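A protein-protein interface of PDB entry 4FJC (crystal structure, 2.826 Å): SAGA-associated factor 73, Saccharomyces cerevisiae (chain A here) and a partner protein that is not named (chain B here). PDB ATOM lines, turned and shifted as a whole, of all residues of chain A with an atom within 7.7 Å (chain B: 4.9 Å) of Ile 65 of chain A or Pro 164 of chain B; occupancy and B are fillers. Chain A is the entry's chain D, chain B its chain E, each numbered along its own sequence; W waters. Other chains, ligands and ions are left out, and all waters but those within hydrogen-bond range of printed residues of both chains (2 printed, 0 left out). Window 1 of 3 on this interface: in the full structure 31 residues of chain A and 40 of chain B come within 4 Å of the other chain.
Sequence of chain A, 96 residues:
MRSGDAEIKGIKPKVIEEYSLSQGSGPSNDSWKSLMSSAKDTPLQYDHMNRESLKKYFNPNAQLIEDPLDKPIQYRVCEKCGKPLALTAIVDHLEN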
ATOM      1  N   TYR A  46     -13.307  29.288  20.217  1.00  0.00           N
ATOM      2  CA  TYR A  46     -12.838  27.945  20.504  1.00  0.00           C
ATOM      3  C   TYR A  46     -11.447  27.781  19.939  1.00  0.00           C
ATOM      4  O   TYR A  46     -11.059  28.442  19.003  1.00  0.00           O
ATOM      5  CB  TYR A  46     -13.764  26.913  19.890  1.00  0.00           C
ATOM      6  CG  TYR A  46     -15.212  27.120  20.244  1.00  0.00           C
ATOM      7  CD1 TYR A  46     -15.690  26.833  21.502  1.00  0.00           C
ATOM      8  CD2 TYR A  46     -16.100  27.614  19.315  1.00  0.00           C
ATOM      9  CE1 TYR A  46     -17.020  27.033  21.840  1.00  0.00           C
ATOM     10  CE2 TYR A  46     -17.433  27.808  19.635  1.00  0.00           C
ATOM     11  CZ  TYR A  46     -17.888  27.514  20.905  1.00  0.00           C
ATOM     12  OH  TYR A  46     -19.221  27.712  21.194  1.00  0.00           O
ATOM     13  N   MET A  49     -11.985  25.359  16.750  1.00  0.00           N
ATOM     14  CA  MET A  49     -13.187  25.378  15.950  1.00  0.00           C
ATOM     15  C   MET A  49     -13.237  26.751  15.317  1.00  0.00           C
ATOM     16  O   MET A  49     -13.711  27.707  15.921  1.00  0.00           O
ATOM     17  CB  MET A  49     -14.428  25.023  16.778  1.00  0.00           C
ATOM     18  CG  MET A  49     -14.557  23.529  17.002  1.00  0.00           C
ATOM     19  SD  MET A  49     -15.935  23.081  18.050  1.00  0.00           S
ATOM     20  CE  MET A  49     -15.403  21.433  18.500  1.00  0.00           C
ATOM     21  N   ALA A  62     -26.170  26.400  16.604  1.00  0.00           N
ATOM     22  CA  ALA A  62     -25.519  25.176  17.044  1.00  0.00           C
ATOM     23  C   ALA A  62     -24.970  25.302  18.456  1.00  0.00           C
ATOM     24  O   ALA A  62     -24.287  26.291  18.770  1.00  0.00           O
ATOM     25  CB  ALA A  62     -24.400  24.827  16.092  1.00  0.00           C
ATOM     26  N   GLN A  63     -25.281  24.312  19.303  1.00  0.00           N
ATOM     27  CA  GLN A  63     -24.533  24.076  20.558  1.00  0.00           C
ATOM     28  C   GLN A  63     -23.177  23.421  20.288  1.00  0.00           C
ATOM     29  O   GLN A  63     -23.088  22.521  19.490  1.00  0.00           O
ATOM     30  CB  GLN A  63     -25.303  23.162  21.504  1.00  0.00           C
ATOM     31  CG  GLN A  63     -26.403  23.825  22.325  1.00  0.00           C
ATOM     32  CD  GLN A  63     -26.984  22.883  23.380  1.00  0.00           C
ATOM     33  OE1 GLN A  63     -26.256  22.113  24.003  1.00  0.00           O
ATOM     34  NE2 GLN A  63     -28.295  22.926  23.568  1.00  0.00           N
ATOM     35  N   LEU A  64     -22.134  23.871  20.970  1.00  0.00           N
ATOM     36  CA  LEU A  64     -20.793  23.313  20.835  1.00  0.00           C
ATOM     37  C   LEU A  64     -20.142  23.098  22.210  1.00  0.00           C
ATOM     38  O   LEU A  64     -20.296  23.932  23.110  1.00  0.00           O
ATOM     39  CB  LEU A  64     -19.927  24.248  20.002  1.00  0.00           C
ATOM     40  CG  LEU A  64     -20.392  24.502  18.553  1.00  0.00           C
ATOM     41  CD1 LEU A  64     -19.679  25.687  17.897  1.00  0.00           C
ATOM     42  CD2 LEU A  64     -20.258  23.245  17.697  1.00  0.00           C
ATOM     43  N   ILE A  65     -19.442  21.970  22.379  1.00  0.00           N
ATOM     44  CA  ILE A  65     -18.592  21.737  23.548  1.00  0.00           C
ATOM     45  C   ILE A  65     -17.227  21.303  23.049  1.00  0.00           C
ATOM     46  O   ILE A  65     -17.114  20.206  22.489  1.00  0.00           O
ATOM     47  CB  ILE A  65     -19.140  20.614  24.462  1.00  0.00           C
ATOM     48  CG1 ILE A  65     -20.558  20.917  24.940  1.00  0.00           C
ATOM     49  CG2 ILE A  65     -18.240  20.422  25.673  1.00  0.00           C
ATOM     50  CD1 ILE A  65     -21.155  19.842  25.823  1.00  0.00           C
ATOM     51  N   GLU A  66     -16.191  22.121  23.266  1.00  0.00           N
ATOM     52  CA  GLU A  66     -14.826  21.769  22.818  1.00  0.00           C
ATOM     53  C   GLU A  66     -14.207  20.691  23.679  1.00  0.00           C
ATOM     54  O   GLU A  66     -14.316  20.758  24.875  1.00  0.00           O
ATOM     55  CB  GLU A  66     -13.891  22.981  22.814  1.00  0.00           C
ATOM     56  CG  GLU A  66     -12.679  22.812  21.889  1.00  0.00           C
ATOM     57  CD  GLU A  66     -11.995  24.131  21.561  1.00  0.00           C
ATOM     58  OE1 GLU A  66     -11.371  24.246  20.458  1.00  0.00           O
ATOM     59  OE2 GLU A  66     -12.098  25.065  22.413  1.00  0.00           O
ATOM     60  N   ASP A  67     -13.552  19.722  23.044  1.00  0.00           N
ATOM     61  CA  ASP A  67     -12.949  18.555  23.689  1.00  0.00           C
ATOM     62  C   ASP A  67     -13.849  17.957  24.753  1.00  0.00           C
ATOM     63  O   ASP A  67     -13.518  17.961  25.927  1.00  0.00           O
ATOM     64  CB  ASP A  67     -11.577  18.917  24.236  1.00  0.00           C
ATOM     65  CG  ASP A  67     -10.595  19.351  23.128  1.00  0.00           C
ATOM     66  OD1 ASP A  67     -10.741  18.872  21.966  1.00  0.00           O
ATOM     67  OD2 ASP A  67      -9.681  20.185  23.392  1.00  0.00           O
ATOM     68  N   PRO A  68     -15.018  17.443  24.344  1.00  0.00           N
ATOM     69  CA  PRO A  68     -16.059  17.034  25.300  1.00  0.00           C
ATOM     70  C   PRO A  68     -15.627  15.989  26.312  1.00  0.00           C
ATOM     71  O   PRO A  68     -16.219  15.910  27.380  1.00  0.00           O
ATOM     72  CB  PRO A  68     -17.155  16.420  24.404  1.00  0.00           C
ATOM     73  CG  PRO A  68     -16.951  17.015  23.059  1.00  0.00           C
ATOM     74  CD  PRO A  68     -15.477  17.338  22.944  1.00  0.00           C
ATOM     75  N   LEU A  69     -14.650  15.161  25.967  1.00  0.00           N
ATOM     76  CA  LEU A  69     -14.217  14.074  26.857  1.00  0.00           C
ATOM     77  C   LEU A  69     -12.820  14.340  27.443  1.00  0.00           C
ATOM     78  O   LEU A  69     -12.191  13.445  28.039  1.00  0.00           O
ATOM     79  CB  LEU A  69     -14.255  12.737  26.100  1.00  0.00           C
ATOM     80  CG  LEU A  69     -15.618  12.025  25.997  1.00  0.00           C
ATOM     81  CD1 LEU A  69     -16.789  12.962  25.721  1.00  0.00           C
ATOM     82  CD2 LEU A  69     -15.536  10.930  24.946  1.00  0.00           C
ATOM     83  N   ILE A  73     -17.067  15.076  33.843  1.00  0.00           N
ATOM     84  CA  ILE A  73     -18.155  16.035  33.906  1.00  0.00           C
ATOM     85  C   ILE A  73     -17.952  16.827  35.151  1.00  0.00           C
ATOM     86  O   ILE A  73     -17.770  16.223  36.206  1.00  0.00           O
ATOM     87  CB  ILE A  73     -19.541  15.411  34.061  1.00  0.00           C
ATOM     88  CG1 ILE A  73     -19.706  14.118  33.258  1.00  0.00           C
ATOM     89  CG2 ILE A  73     -20.562  16.431  33.642  1.00  0.00           C
ATOM     90  CD1 ILE A  73     -21.117  13.596  33.351  1.00  0.00           C
ATOM     91  N   HIS B 162     -24.464   9.018  28.102  1.00  0.00           N
ATOM     92  CA  HIS B 162     -23.004   9.216  28.015  1.00  0.00           C
ATOM     93  C   HIS B 162     -22.689  10.150  26.911  1.00  0.00           C
ATOM     94  O   HIS B 162     -21.640  10.085  26.257  1.00  0.00           O
ATOM     95  CB  HIS B 162     -22.277   7.886  27.860  1.00  0.00           C
ATOM     96  CG  HIS B 162     -22.242   7.113  29.127  1.00  0.00           C
ATOM     97  ND1 HIS B 162     -23.162   6.179  29.432  1.00  0.00           N
ATOM     98  CD2 HIS B 162     -21.437   7.244  30.229  1.00  0.00           C
ATOM     99  CE1 HIS B 162     -22.908   5.693  30.646  1.00  0.00           C
ATOM    100  NE2 HIS B 162     -21.851   6.353  31.138  1.00  0.00           N
ATOM    101  N   ASN B 163     -23.620  11.051  26.702  1.00  0.00           N
ATOM    102  CA  ASN B 163     -23.517  11.995  25.652  1.00  0.00           C
ATOM    103  C   ASN B 163     -23.375  13.372  26.319  1.00  0.00           C
ATOM    104  O   ASN B 163     -24.289  13.855  27.002  1.00  0.00           O
ATOM    105  CB  ASN B 163     -24.726  11.878  24.739  1.00  0.00           C
ATOM    106  CG  ASN B 163     -24.739  12.950  23.698  1.00  0.00           C
ATOM    107  OD1 ASN B 163     -24.865  14.114  24.033  1.00  0.00           O
ATOM    108  ND2 ASN B 163     -24.589  12.582  22.448  1.00  0.00           N
ATOM    109  N   PRO B 164     -22.212  14.002  26.120  1.00  0.00           N
ATOM    110  CA  PRO B 164     -21.888  15.208  26.853  1.00  0.00           C
ATOM    111  C   PRO B 164     -22.896  16.310  26.645  1.00  0.00           C
ATOM    112  O   PRO B 164     -23.121  17.089  27.569  1.00  0.00           O
ATOM    113  CB  PRO B 164     -20.538  15.628  26.284  1.00  0.00           C
ATOM    114  CG  PRO B 164     -19.999  14.431  25.583  1.00  0.00           C
ATOM    115  CD  PRO B 164     -21.206  13.703  25.081  1.00  0.00           C
ATOM    116  N   TYR B 165     -23.514  16.389  25.473  1.00  0.00           N
ATOM    117  CA  TYR B 165     -24.504  17.446  25.233  1.00  0.00           C
ATOM    118  C   TYR B 165     -25.790  17.238  25.999  1.00  0.00           C
ATOM    119  O   TYR B 165     -26.363  18.185  26.514  1.00  0.00           O
ATOM    120  CB  TYR B 165     -24.811  17.577  23.756  1.00  0.00           C
ATOM    121  CG  TYR B 165     -23.671  18.182  22.992  1.00  0.00           C
ATOM    122  CD1 TYR B 165     -23.593  19.536  22.822  1.00  0.00           C
ATOM    123  CD2 TYR B 165     -22.694  17.397  22.437  1.00  0.00           C
ATOM    124  CE1 TYR B 165     -22.562  20.106  22.118  1.00  0.00           C
ATOM    125  CE2 TYR B 165     -21.656  17.956  21.736  1.00  0.00           C
ATOM    126  CZ  TYR B 165     -21.594  19.317  21.590  1.00  0.00           C
ATOM    127  OH  TYR B 165     -20.564  19.908  20.906  1.00  0.00           O
ATOM    128  N   PHE B 166     -26.240  15.994  26.079  1.00  0.00           N
ATOM    129  CA  PHE B 166     -27.440  15.679  26.844  1.00  0.00           C
ATOM    130  C   PHE B 166     -27.183  15.678  28.351  1.00  0.00           C
ATOM    131  O   PHE B 166     -27.960  16.246  29.111  1.00  0.00           O
ATOM    132  CB  PHE B 166     -28.030  14.337  26.427  1.00  0.00           C
ATOM    133  CG  PHE B 166     -29.284  14.011  27.158  1.00  0.00           C
ATOM    134  CD1 PHE B 166     -30.484  14.619  26.797  1.00  0.00           C
ATOM    135  CD2 PHE B 166     -29.266  13.153  28.268  1.00  0.00           C
ATOM    136  CE1 PHE B 166     -31.658  14.359  27.509  1.00  0.00           C
ATOM    137  CE2 PHE B 166     -30.438  12.902  28.990  1.00  0.00           C
ATOM    138  CZ  PHE B 166     -31.636  13.503  28.606  1.00  0.00           C
ATOM    139  N   ILE B 167     -26.117  15.029  28.796  1.00  0.00           N
ATOM    140  CA  ILE B 167     -25.755  15.092  30.212  1.00  0.00           C
ATOM    141  C   ILE B 167     -25.808  16.545  30.646  1.00  0.00           C
ATOM    142  O   ILE B 167     -26.459  16.885  31.627  1.00  0.00           O
ATOM    143  CB  ILE B 167     -24.338  14.524  30.461  1.00  0.00           C
ATOM    144  CG1 ILE B 167     -24.347  12.991  30.328  1.00  0.00           C
ATOM    145  CG2 ILE B 167     -23.798  14.884  31.842  1.00  0.00           C
ATOM    146  CD1 ILE B 167     -23.021  12.427  29.809  1.00  0.00           C
ATOM    147  N   ARG B 168     -25.132  17.409  29.889  1.00  0.00           N
ATOM    148  CA  ARG B 168     -25.100  18.849  30.202  1.00  0.00           C
ATOM    149  C   ARG B 168     -26.472  19.467  30.229  1.00  0.00           C
ATOM    150  O   ARG B 168     -26.770  20.266  31.090  1.00  0.00           O
ATOM    151  CB  ARG B 168     -24.258  19.628  29.199  1.00  0.00           C
ATOM    152  CG  ARG B 168     -24.073  21.061  29.639  1.00  0.00           C
ATOM    153  CD  ARG B 168     -23.206  21.851  28.678  1.00  0.00           C
ATOM    154  NE  ARG B 168     -23.812  22.016  27.350  1.00  0.00           N
ATOM    155  CZ  ARG B 168     -23.327  22.800  26.399  1.00  0.00           C
ATOM    156  NH1 ARG B 168     -22.243  23.512  26.614  1.00  0.00           N
ATOM    157  NH2 ARG B 168     -23.938  22.876  25.238  1.00  0.00           N
ATOM    158  N   ILE B 419     -17.682   8.313  19.773  1.00  0.00           N
ATOM    159  CA  ILE B 419     -17.914   8.169  21.228  1.00  0.00           C
ATOM    160  C   ILE B 419     -19.001   7.184  21.592  1.00  0.00           C
ATOM    161  O   ILE B 419     -19.295   7.045  22.777  1.00  0.00           O
ATOM    162  CB  ILE B 419     -18.301   9.494  21.920  1.00  0.00           C
ATOM    163  CG1 ILE B 419     -19.705   9.920  21.494  1.00  0.00           C
ATOM    164  CG2 ILE B 419     -17.299  10.589  21.604  1.00  0.00           C
ATOM    165  CD1 ILE B 419     -20.067  11.302  21.968  1.00  0.00           C
ATOM    166  N   ILE B 472     -18.394  16.290  17.476  1.00  0.00           N
ATOM    167  CA  ILE B 472     -17.529  17.221  16.738  1.00  0.00           C
ATOM    168  C   ILE B 472     -16.345  17.601  17.599  1.00  0.00           C
ATOM    169  O   ILE B 472     -16.488  17.861  18.794  1.00  0.00           O
ATOM    170  CB  ILE B 472     -18.267  18.490  16.226  1.00  0.00           C
ATOM    171  CG1 ILE B 472     -17.390  19.262  15.222  1.00  0.00           C
ATOM    172  CG2 ILE B 472     -18.647  19.424  17.355  1.00  0.00           C
ATOM    173  CD1 ILE B 472     -16.832  18.455  14.065  1.00  0.00           C
HETATM  174  O   HOH W   1     -18.288  18.565  20.723  1.00  0.00           O
HETATM  175  O   HOH W   2     -26.132  20.560  26.063  1.00  0.00           O
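Ile 65 of chain A touches just these residues of chain B: Pro 164 (3.8 Å), Tyr 165 (2.8 Å) and Arg 168 (3.5 Å).
Pro 164 of chain B touches just these residues of chain A: Ile 65, Pro 68 and Leu 69.
Printed residues of chain B within 4 Å of Pro 68 of chain A: Pro 164 (3.7 Å).
Printed residues of chain A within 4 Å of Ile 419 of chain B: Leu 69.
Printed residues of chain A within 4 Å of Ile 472 of chain B: Met 49 (3.7 Å).
Printed residues of chain B within 4 Å of Gln 63 of chain A: Tyr 165 and Arg 168.
His 162 of chain B touches none of the printed residues of chain A.
The nearest printed residue of chain A that does not touch Ile 419 of chain B is Pro 68 of chain A (6.4 Å).
OD1 of Asn 163 of chain B sits at hydrogen-bond distance from N of Tyr 165 of chain B (3.0 Å).
Among the printed residues, pairs that only touch across the chains: Met 49 of chain A with Ile 472 of chain B, Gln 63 of chain A with Tyr 165 of chain B, Leu 64 of chain A with Tyr 165 of chain B, Ile 65 of chain A with Pro 164 of chain B, Ile 65 of chain A with Arg 168 of chain B, Pro 68 of chain A with Pro 164 of chain B, Leu 69 of chain A with Pro 164 of chain B, Leu 69 of chain A with Ile 419 of chain B and Ile 73 of chain A with Ile 167 of chain B.
Water W2 lies within hydrogen-bond range of O of Tyr 165 of chain B, OE1 of Gln 63 of chain A and NE of Arg 168 of chain B.
Water W1 lies within hydrogen-bond range of OH of Tyr 165 of chain B (2.6 Å), O of Ile 65 of chain A (2.7 Å) and O of Ile 472 of chain B (2.7 Å).
OH of Tyr 165 of chain B is in hydrogen-bond range of N of Ile 65 of chain A (2.8 Å).
The side-chain amide oxygen (OE1) of Gln 63 of chain A lies within hydrogen-bond range of the guanidinium group (NH2) of Arg 168 of chain B, 2.7 Å away.
Of the 11 printed residues of chain A, 7 touch a printed residue of chain B.
Printed residues of chain A that touch a printed residue of chain B: Met 49, Gln 63, Leu 64, Ile 65, Pro 68, Leu 69 and Ile 73.
Along chain A the printed residues that touch a printed residue of chain B span positions 49 to 73.
Of the 9 printed residues of chain B, 6 touch a printed residue of chain A.
Hydrophobic or aromatic side chains of chain B within 4 Å of the printed part of chain A: Pro 164, Tyr 165, Ile 167, Ile 419 and Ile 472.
Among the printed residues, no Asp or Glu carboxylate lies within 4 Å of a Lys or Arg side-chain nitrogen of the other chain.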
